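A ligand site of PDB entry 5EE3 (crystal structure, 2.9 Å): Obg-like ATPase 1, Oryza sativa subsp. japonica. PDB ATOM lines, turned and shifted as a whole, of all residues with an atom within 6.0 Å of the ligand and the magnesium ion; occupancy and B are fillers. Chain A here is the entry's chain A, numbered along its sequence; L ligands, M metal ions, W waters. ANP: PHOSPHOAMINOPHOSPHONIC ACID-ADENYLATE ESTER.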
ATOM      1  N   GLY A  32      -2.786   5.379 -10.255  1.00  0.00           N
ATOM      2  CA  GLY A  32      -1.407   4.906 -10.114  1.00  0.00           C
ATOM      3  C   GLY A  32      -1.247   3.432 -10.439  1.00  0.00           C
ATOM      4  O   GLY A  32      -2.246   2.731 -10.614  1.00  0.00           O
ATOM      5  N   LEU A  33      -0.007   2.959 -10.514  1.00  0.00           N
ATOM      6  CA  LEU A  33       0.279   1.539 -10.785  1.00  0.00           C
ATOM      7  C   LEU A  33      -0.071   0.682  -9.547  1.00  0.00           C
ATOM      8  O   LEU A  33      -0.101   1.214  -8.433  1.00  0.00           O
ATOM      9  CB  LEU A  33       1.734   1.338 -11.205  1.00  0.00           C
ATOM     10  N   PRO A  34      -0.343  -0.629  -9.746  1.00  0.00           N
ATOM     11  CA  PRO A  34      -0.745  -1.461  -8.597  1.00  0.00           C
ATOM     12  C   PRO A  34       0.293  -1.543  -7.469  1.00  0.00           C
ATOM     13  O   PRO A  34       1.499  -1.597  -7.743  1.00  0.00           O
ATOM     14  CB  PRO A  34      -0.985  -2.838  -9.231  1.00  0.00           C
ATOM     15  CG  PRO A  34      -1.316  -2.548 -10.647  1.00  0.00           C
ATOM     16  CD  PRO A  34      -0.465  -1.365 -11.013  1.00  0.00           C
ATOM     17  N   ASN A  35      -0.195  -1.559  -6.226  1.00  0.00           N
ATOM     18  CA  ASN A  35       0.641  -1.595  -5.020  1.00  0.00           C
ATOM     19  C   ASN A  35       1.752  -0.527  -4.994  1.00  0.00           C
ATOM     20  O   ASN A  35       2.948  -0.849  -4.978  1.00  0.00           O
ATOM     21  CB  ASN A  35       1.188  -2.997  -4.790  1.00  0.00           C
ATOM     22  CG  ASN A  35       0.094  -4.050  -4.742  1.00  0.00           C
ATOM     23  OD1 ASN A  35      -1.088  -3.725  -4.578  1.00  0.00           O
ATOM     24  ND2 ASN A  35       0.476  -5.318  -4.907  1.00  0.00           N
ATOM     25  N   VAL A  36       1.312   0.723  -5.034  1.00  0.00           N
ATOM     26  CA  VAL A  36       2.164   1.903  -4.796  1.00  0.00           C
ATOM     27  C   VAL A  36       1.708   2.751  -3.593  1.00  0.00           C
ATOM     28  O   VAL A  36       2.431   3.669  -3.187  1.00  0.00           O
ATOM     29  CB  VAL A  36       2.277   2.824  -6.046  1.00  0.00           C
ATOM     30  CG1 VAL A  36       2.882   2.058  -7.227  1.00  0.00           C
ATOM     31  CG2 VAL A  36       0.927   3.450  -6.426  1.00  0.00           C
ATOM     32  N   GLY A  37       0.545   2.424  -3.013  1.00  0.00           N
ATOM     33  CA  GLY A  37      -0.026   3.207  -1.902  1.00  0.00           C
ATOM     34  C   GLY A  37      -1.429   3.766  -2.093  1.00  0.00           C
ATOM     35  O   GLY A  37      -1.893   4.498  -1.226  1.00  0.00           O
ATOM     36  N   LYS A  38      -2.113   3.395  -3.176  1.00  0.00           N
ATOM     37  CA  LYS A  38      -3.407   4.001  -3.531  1.00  0.00           C
ATOM     38  C   LYS A  38      -4.499   3.812  -2.459  1.00  0.00           C
ATOM     39  O   LYS A  38      -5.109   4.789  -2.032  1.00  0.00           O
ATOM     40  CB  LYS A  38      -3.918   3.456  -4.881  1.00  0.00           C
ATOM     41  CG  LYS A  38      -3.058   3.819  -6.089  1.00  0.00           C
ATOM     42  CD  LYS A  38      -3.558   3.123  -7.358  1.00  0.00           C
ATOM     43  CE  LYS A  38      -4.776   3.839  -7.929  1.00  0.00           C
ATOM     44  NZ  LYS A  38      -5.354   3.204  -9.145  1.00  0.00           N
ATOM     45  N   SER A  39      -4.728   2.563  -2.036  1.00  0.00           N
ATOM     46  CA  SER A  39      -5.743   2.275  -0.996  1.00  0.00           C
ATOM     47  C   SER A  39      -5.265   2.676   0.385  1.00  0.00           C
ATOM     48  O   SER A  39      -6.060   3.152   1.182  1.00  0.00           O
ATOM     49  CB  SER A  39      -6.183   0.814  -0.986  1.00  0.00           C
ATOM     50  OG  SER A  39      -6.994   0.503  -2.103  1.00  0.00           O
ATOM     51  N   THR A  40      -3.970   2.507   0.660  1.00  0.00           N
ATOM     52  CA  THR A  40      -3.399   2.950   1.935  1.00  0.00           C
ATOM     53  C   THR A  40      -3.569   4.465   2.131  1.00  0.00           C
ATOM     54  O   THR A  40      -3.906   4.924   3.230  1.00  0.00           O
ATOM     55  CB  THR A  40      -1.927   2.537   2.073  1.00  0.00           C
ATOM     56  OG1 THR A  40      -1.815   1.127   1.838  1.00  0.00           O
ATOM     57  CG2 THR A  40      -1.406   2.825   3.479  1.00  0.00           C
ATOM     58  N   PHE A  41      -3.355   5.241   1.064  1.00  0.00           N
ATOM     59  CA  PHE A  41      -3.653   6.674   1.072  1.00  0.00           C
ATOM     60  C   PHE A  41      -5.154   6.949   1.189  1.00  0.00           C
ATOM     61  O   PHE A  41      -5.561   7.819   1.951  1.00  0.00           O
ATOM     62  CB  PHE A  41      -3.097   7.352  -0.189  1.00  0.00           C
ATOM     63  CG  PHE A  41      -3.531   8.790  -0.361  1.00  0.00           C
ATOM     64  CD1 PHE A  41      -3.106   9.755   0.539  1.00  0.00           C
ATOM     65  CD2 PHE A  41      -4.367   9.161  -1.400  1.00  0.00           C
ATOM     66  CE1 PHE A  41      -3.506  11.075   0.390  1.00  0.00           C
ATOM     67  CE2 PHE A  41      -4.767  10.480  -1.549  1.00  0.00           C
ATOM     68  CZ  PHE A  41      -4.334  11.434  -0.651  1.00  0.00           C
ATOM     69  N   ASP A  95     -11.219   6.521  -4.865  1.00  0.00           N
ATOM     70  CA  ASP A  95     -10.262   5.433  -5.051  1.00  0.00           C
ATOM     71  C   ASP A  95     -10.667   4.695  -6.313  1.00  0.00           C
ATOM     72  O   ASP A  95     -11.780   4.202  -6.401  1.00  0.00           O
ATOM     73  CB  ASP A  95     -10.267   4.480  -3.856  1.00  0.00           C
ATOM     74  CG  ASP A  95      -9.023   3.587  -3.783  1.00  0.00           C
ATOM     75  OD1 ASP A  95      -8.421   3.262  -4.834  1.00  0.00           O
ATOM     76  OD2 ASP A  95      -8.654   3.209  -2.647  1.00  0.00           O
ATOM     77  N   ILE A  96      -9.768   4.660  -7.282  1.00  0.00           N
ATOM     78  CA  ILE A  96      -9.982   3.957  -8.536  1.00  0.00           C
ATOM     79  C   ILE A  96      -9.163   2.666  -8.493  1.00  0.00           C
ATOM     80  O   ILE A  96      -8.059   2.640  -7.930  1.00  0.00           O
ATOM     81  CB  ILE A  96      -9.566   4.817  -9.744  1.00  0.00           C
ATOM     82  CG1 ILE A  96     -10.269   6.187  -9.679  1.00  0.00           C
ATOM     83  CG2 ILE A  96      -9.851   4.086 -11.054  1.00  0.00           C
ATOM     84  CD1 ILE A  96      -9.729   7.204 -10.657  1.00  0.00           C
ATOM     85  N   ALA A  97      -9.728   1.600  -9.075  1.00  0.00           N
ATOM     86  CA  ALA A  97      -9.096   0.273  -9.162  1.00  0.00           C
ATOM     87  C   ALA A  97      -8.541  -0.217  -7.823  1.00  0.00           C
ATOM     88  O   ALA A  97      -9.212  -0.142  -6.795  1.00  0.00           O
ATOM     89  CB  ALA A  97      -8.021   0.258 -10.234  1.00  0.00           C
ATOM     90  N   LEU A 109      -3.786   0.607 -16.210  1.00  0.00           N
ATOM     91  CA  LEU A 109      -4.125  -0.585 -15.433  1.00  0.00           C
ATOM     92  C   LEU A 109      -5.139  -1.487 -16.161  1.00  0.00           C
ATOM     93  O   LEU A 109      -5.045  -2.722 -16.056  1.00  0.00           O
ATOM     94  CB  LEU A 109      -4.670  -0.186 -14.059  1.00  0.00           C
ATOM     95  CG  LEU A 109      -4.844  -1.310 -13.032  1.00  0.00           C
ATOM     96  N   PHE A 130       9.966   4.226  -2.875  1.00  0.00           N
ATOM     97  CA  PHE A 130      10.579   3.475  -1.768  1.00  0.00           C
ATOM     98  C   PHE A 130      10.901   2.045  -2.192  1.00  0.00           C
ATOM     99  O   PHE A 130      10.197   1.469  -3.040  1.00  0.00           O
ATOM    100  CB  PHE A 130       9.676   3.484  -0.524  1.00  0.00           C
ATOM    101  CG  PHE A 130       8.335   2.828  -0.736  1.00  0.00           C
ATOM    102  CD1 PHE A 130       7.278   3.516  -1.340  1.00  0.00           C
ATOM    103  CD2 PHE A 130       8.107   1.519  -0.303  1.00  0.00           C
ATOM    104  CE1 PHE A 130       6.047   2.908  -1.529  1.00  0.00           C
ATOM    105  CE2 PHE A 130       6.867   0.905  -0.493  1.00  0.00           C
ATOM    106  CZ  PHE A 130       5.839   1.605  -1.101  1.00  0.00           C
ATOM    107  N   ASN A 231       5.128   8.874  -2.982  1.00  0.00           N
ATOM    108  CA  ASN A 231       5.138   8.016  -1.799  1.00  0.00           C
ATOM    109  C   ASN A 231       6.543   7.505  -1.484  1.00  0.00           C
ATOM    110  O   ASN A 231       7.225   6.981  -2.369  1.00  0.00           O
ATOM    111  CB  ASN A 231       4.203   6.827  -1.995  1.00  0.00           C
ATOM    112  CG  ASN A 231       3.998   6.000  -0.744  1.00  0.00           C
ATOM    113  OD1 ASN A 231       4.480   6.353   0.343  1.00  0.00           O
ATOM    114  ND2 ASN A 231       3.276   4.891  -0.874  1.00  0.00           N
ATOM    115  N   MET A 232       6.969   7.649  -0.227  1.00  0.00           N
ATOM    116  CA  MET A 232       8.317   7.251   0.193  1.00  0.00           C
ATOM    117  C   MET A 232       8.359   6.790   1.648  1.00  0.00           C
ATOM    118  O   MET A 232       7.355   6.853   2.363  1.00  0.00           O
ATOM    119  CB  MET A 232       9.286   8.424  -0.022  1.00  0.00           C
ATOM    120  CG  MET A 232       8.998   9.638   0.845  1.00  0.00           C
ATOM    121  SD  MET A 232       9.983  11.091   0.435  1.00  0.00           S
ATOM    122  CE  MET A 232       9.531  11.348  -1.282  1.00  0.00           C
ATOM    123  N   SER A 233       9.531   6.327   2.099  1.00  0.00           N
ATOM    124  CA  SER A 233       9.716   5.915   3.493  1.00  0.00           C
ATOM    125  C   SER A 233       9.475   7.095   4.440  1.00  0.00           C
ATOM    126  O   SER A 233       9.567   8.252   4.043  1.00  0.00           O
ATOM    127  CB  SER A 233      11.126   5.336   3.723  1.00  0.00           C
ATOM    128  OG  SER A 233      12.099   6.345   3.931  1.00  0.00           O
ATOM    129  N   GLU A 234       9.129   6.788   5.683  1.00  0.00           N
ATOM    130  CA  GLU A 234       9.034   7.806   6.732  1.00  0.00           C
ATOM    131  C   GLU A 234      10.391   8.468   6.975  1.00  0.00           C
ATOM    132  O   GLU A 234      10.464   9.664   7.260  1.00  0.00           O
ATOM    133  CB  GLU A 234       8.514   7.177   8.031  1.00  0.00           C
ATOM    134  CG  GLU A 234       8.545   8.109   9.253  1.00  0.00           C
ATOM    135  CD  GLU A 234       7.919   7.491  10.496  1.00  0.00           C
ATOM    136  OE1 GLU A 234       7.457   6.332  10.430  1.00  0.00           O
ATOM    137  OE2 GLU A 234       7.898   8.176  11.537  1.00  0.00           O
ATOM    138  N   PHE A 263       5.397  12.581   0.257  1.00  0.00           N
ATOM    139  CA  PHE A 263       4.722  12.089   1.464  1.00  0.00           C
ATOM    140  C   PHE A 263       5.093  10.637   1.741  1.00  0.00           C
ATOM    141  O   PHE A 263       5.475   9.895   0.829  1.00  0.00           O
ATOM    142  CB  PHE A 263       3.190  12.267   1.348  1.00  0.00           C
ATOM    143  CG  PHE A 263       2.476  11.169   0.602  1.00  0.00           C
ATOM    144  CD1 PHE A 263       2.797  10.872  -0.713  1.00  0.00           C
ATOM    145  CD2 PHE A 263       1.468  10.426   1.224  1.00  0.00           C
ATOM    146  CE1 PHE A 263       2.136   9.846  -1.388  1.00  0.00           C
ATOM    147  CE2 PHE A 263       0.815   9.405   0.549  1.00  0.00           C
ATOM    148  CZ  PHE A 263       1.142   9.118  -0.756  1.00  0.00           C
ATOM    149  N   SER A 264       4.992  10.236   3.004  1.00  0.00           N
ATOM    150  CA  SER A 264       5.138   8.842   3.390  1.00  0.00           C
ATOM    151  C   SER A 264       3.773   8.288   3.769  1.00  0.00           C
ATOM    152  O   SER A 264       3.170   8.746   4.730  1.00  0.00           O
ATOM    153  CB  SER A 264       6.114   8.681   4.561  1.00  0.00           C
ATOM    154  OG  SER A 264       6.170   7.329   5.003  1.00  0.00           O
ATOM    155  N   CYS A 265       3.319   7.304   3.017  1.00  0.00           N
ATOM    156  CA  CYS A 265       2.041   6.643   3.299  1.00  0.00           C
ATOM    157  C   CYS A 265       2.054   5.890   4.623  1.00  0.00           C
ATOM    158  O   CYS A 265       1.048   5.860   5.329  1.00  0.00           O
ATOM    159  CB  CYS A 265       1.670   5.693   2.165  1.00  0.00           C
ATOM    160  SG  CYS A 265      -0.086   5.688   1.799  1.00  0.00           S
ATOM    161  N   ALA A 266       3.201   5.293   4.978  1.00  0.00           N
ATOM    162  CA  ALA A 266       3.349   4.559   6.242  1.00  0.00           C
ATOM    163  C   ALA A 266       3.233   5.483   7.461  1.00  0.00           C
ATOM    164  O   ALA A 266       2.431   5.235   8.367  1.00  0.00           O
ATOM    165  CB  ALA A 266       4.671   3.815   6.278  1.00  0.00           C
ATOM    166  N   PHE A 267       4.041   6.551   7.456  1.00  0.00           N
ATOM    167  CA  PHE A 267       3.995   7.563   8.519  1.00  0.00           C
ATOM    168  C   PHE A 267       2.593   8.119   8.744  1.00  0.00           C
ATOM    169  O   PHE A 267       2.160   8.266   9.880  1.00  0.00           O
ATOM    170  CB  PHE A 267       4.934   8.727   8.194  1.00  0.00           C
ATOM    171  CG  PHE A 267       4.693   9.968   9.030  1.00  0.00           C
ATOM    172  CD1 PHE A 267       4.888   9.947  10.400  1.00  0.00           C
ATOM    173  CD2 PHE A 267       4.242  11.146   8.439  1.00  0.00           C
ATOM    174  CE1 PHE A 267       4.648  11.081  11.174  1.00  0.00           C
ATOM    175  CE2 PHE A 267       4.014  12.283   9.193  1.00  0.00           C
ATOM    176  CZ  PHE A 267       4.217  12.250  10.560  1.00  0.00           C
ATOM    177  N   ARG A 269      -0.399   6.834   7.804  1.00  0.00           N
ATOM    178  CA  ARG A 269      -1.201   5.699   8.314  1.00  0.00           C
ATOM    179  C   ARG A 269      -1.007   5.520   9.814  1.00  0.00           C
ATOM    180  O   ARG A 269      -1.962   5.437  10.575  1.00  0.00           O
ATOM    181  CB  ARG A 269      -0.811   4.409   7.578  1.00  0.00           C
ATOM    182  CG  ARG A 269      -1.487   3.131   8.057  1.00  0.00           C
ATOM    183  CD  ARG A 269      -1.029   1.940   7.231  1.00  0.00           C
ATOM    184  NE  ARG A 269      -1.816   0.745   7.509  1.00  0.00           N
ATOM    185  CZ  ARG A 269      -2.995   0.485   6.965  1.00  0.00           C
ATOM    186  NH2 ARG A 269      -3.649  -0.625   7.280  1.00  0.00           N
HETATM  187  PG  ANP L   1      -4.326  -1.200  -6.703  1.00  0.00           P
HETATM  188  O1G ANP L   1      -5.660  -1.384  -6.013  1.00  0.00           O
HETATM  189  O2G ANP L   1      -4.386  -0.361  -7.962  1.00  0.00           O
HETATM  190  O3G ANP L   1      -3.537  -2.489  -6.825  1.00  0.00           O
HETATM  191  PB  ANP L   1      -3.527  -0.643  -3.933  1.00  0.00           P
HETATM  192  O1B ANP L   1      -4.803   0.011  -3.482  1.00  0.00           O
HETATM  193  O2B ANP L   1      -3.412  -2.142  -3.840  1.00  0.00           O
HETATM  194  N3B ANP L   1      -3.365  -0.244  -5.606  1.00  0.00           N
HETATM  195  PA  ANP L   1      -2.202  -0.366  -1.490  1.00  0.00           P
HETATM  196  O1A ANP L   1      -2.012   0.914  -0.722  1.00  0.00           O
HETATM  197  O2A ANP L   1      -3.319  -1.283  -1.043  1.00  0.00           O
HETATM  198  O3A ANP L   1      -2.337  -0.002  -3.056  1.00  0.00           O
HETATM  199  O5' ANP L   1      -0.848  -1.249  -1.507  1.00  0.00           O
HETATM  200  C5' ANP L   1       0.448  -0.716  -1.281  1.00  0.00           C
HETATM  201  C4' ANP L   1       1.153  -1.568  -0.235  1.00  0.00           C
HETATM  202  O4' ANP L   1       2.455  -1.020  -0.027  1.00  0.00           O
HETATM  203  C3' ANP L   1       0.429  -1.581   1.108  1.00  0.00           C
HETATM  204  O3' ANP L   1       0.288  -2.925   1.579  1.00  0.00           O
HETATM  205  C2' ANP L   1       1.288  -0.735   2.033  1.00  0.00           C
HETATM  206  O2' ANP L   1       1.390  -1.286   3.343  1.00  0.00           O
HETATM  207  C1' ANP L   1       2.644  -0.665   1.344  1.00  0.00           C
HETATM  208  N9  ANP L   1       3.221   0.705   1.441  1.00  0.00           N
HETATM  209  C8  ANP L   1       2.697   1.819   0.903  1.00  0.00           C
HETATM  210  N7  ANP L   1       3.478   2.895   1.193  1.00  0.00           N
HETATM  211  C5  ANP L   1       4.527   2.468   1.915  1.00  0.00           C
HETATM  212  C6  ANP L   1       5.735   3.072   2.534  1.00  0.00           C
HETATM  213  N6  ANP L   1       5.973   4.398   2.434  1.00  0.00           N
HETATM  214  N1  ANP L   1       6.579   2.254   3.214  1.00  0.00           N
HETATM  215  C2  ANP L   1       6.357   0.919   3.327  1.00  0.00           C
HETATM  216  N3  ANP L   1       5.284   0.311   2.787  1.00  0.00           N
HETATM  217  C4  ANP L   1       4.354   1.005   2.077  1.00  0.00           C
HETATM  218 MG    MG M   1      -7.373   0.167  -4.076  1.00  0.00          MG
HETATM  219  O   HOH W   1       1.826   1.437   5.260  1.00  0.00           O
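The backbone NH (N) of Ser 39 sits at hydrogen-bond distance from an oxygen (O1B) of the ligand (2.9 Å).
OG of Ser 39 sits close to O1B of the ligand (2.6 Å).
An oxygen (O1A) of the ligand sits at hydrogen-bond distance from the backbone NH (N) of Thr 40 (2.9 Å).
The side-chain hydroxyl of Thr 40 is in hydrogen-bond range of an oxygen (O1A) of the ligand (2.6 Å).
The backbone carbonyl oxygen (O) of Met 232 is in hydrogen-bond range of a nitrogen (N6) of the ligand (2.8 Å).
ND2 of Asn 231 sits at hydrogen-bond distance from N7 of the ligand, 2.9 Å away.
The side-chain amide oxygen (OD1) of Asn 35 lies close to an oxygen (O2B) of the ligand (2.9 Å).
An oxygen (O3A) of the ligand lies within hydrogen-bond range of the backbone NH (N) of Lys 38 (3.4 Å).
The side-chain amino group (NZ) of Lys 38 is in salt-bridge range of an oxygen (O2G) of the ligand (3.9 Å).
OD2 of Asp 95 sits close to OG of Ser 39 (3.2 Å).
O of Phe 263 is in hydrogen-bond range of N of Met 232 (2.9 Å).
The side-chain amide oxygen (OD1) of Asn 231 is in hydrogen-bond range of the backbone NH (N) of Cys 265 (3.1 Å).
SG of Cys 265 lies within hydrogen-bond range of O of Gly 37, 3.7 Å away.
NZ of Lys 38 sits at hydrogen-bond distance from O of Gly 32.
The backbone carbonyl oxygen (O) of Ile 96 sits at hydrogen-bond distance from the side-chain amino group (NZ) of Lys 38, at 3.0 Å.
The backbone NH of Glu 234 sits at hydrogen-bond distance from the side-chain hydroxyl of Ser 264 (3.1 Å).
The side-chain hydroxyl of Ser 264 sits at hydrogen-bond distance from the backbone NH of Phe 267, 3.3 Å away.
OD1 of Asp 95 touches the magnesium ion, 3.4 Å away.
Ala 97 touches the magnesium ion.
Within 4 Å of the magnesium ion: Ser 39, Asp 95 and Ala 97.
The nearest printed residue that does not touch the magnesium ion is Ile 96 (4.6 Å).
CA of Pro 34 touches O3G of the ligand, 3.5 Å away.
Gly 37 touches the ligand (C to O1A, 3.2 Å).
Ala 97 touches the ligand (C to O1G, 3.6 Å).
Phe 130 touches the ligand.
OG of Ser 264 touches N6 of the ligand, 3.9 Å away.
CB of Cys 265 touches N7 of the ligand, at 3.5 Å.
Ala 266 touches the ligand (N to N6, 3.9 Å).
Hydrophobic or aromatic side chains within 4 Å of the ligand: Pro 34, Phe 130 and Ala 266.
Within 4 Å of the ligand: Pro 34, Asn 35, Gly 37, Lys 38, Ser 39, Thr 40, Ala 97, Phe 130, Asn 231, Met 232, Ser 264, Cys 265 and Ala 266.
The magnesium ion is bound by the side-chain hydroxyl (OG) of Ser 39 (2.0 Å).
Slightly farther from the magnesium ion lies an oxygen (O1B) of the ligand (2.6 Å).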
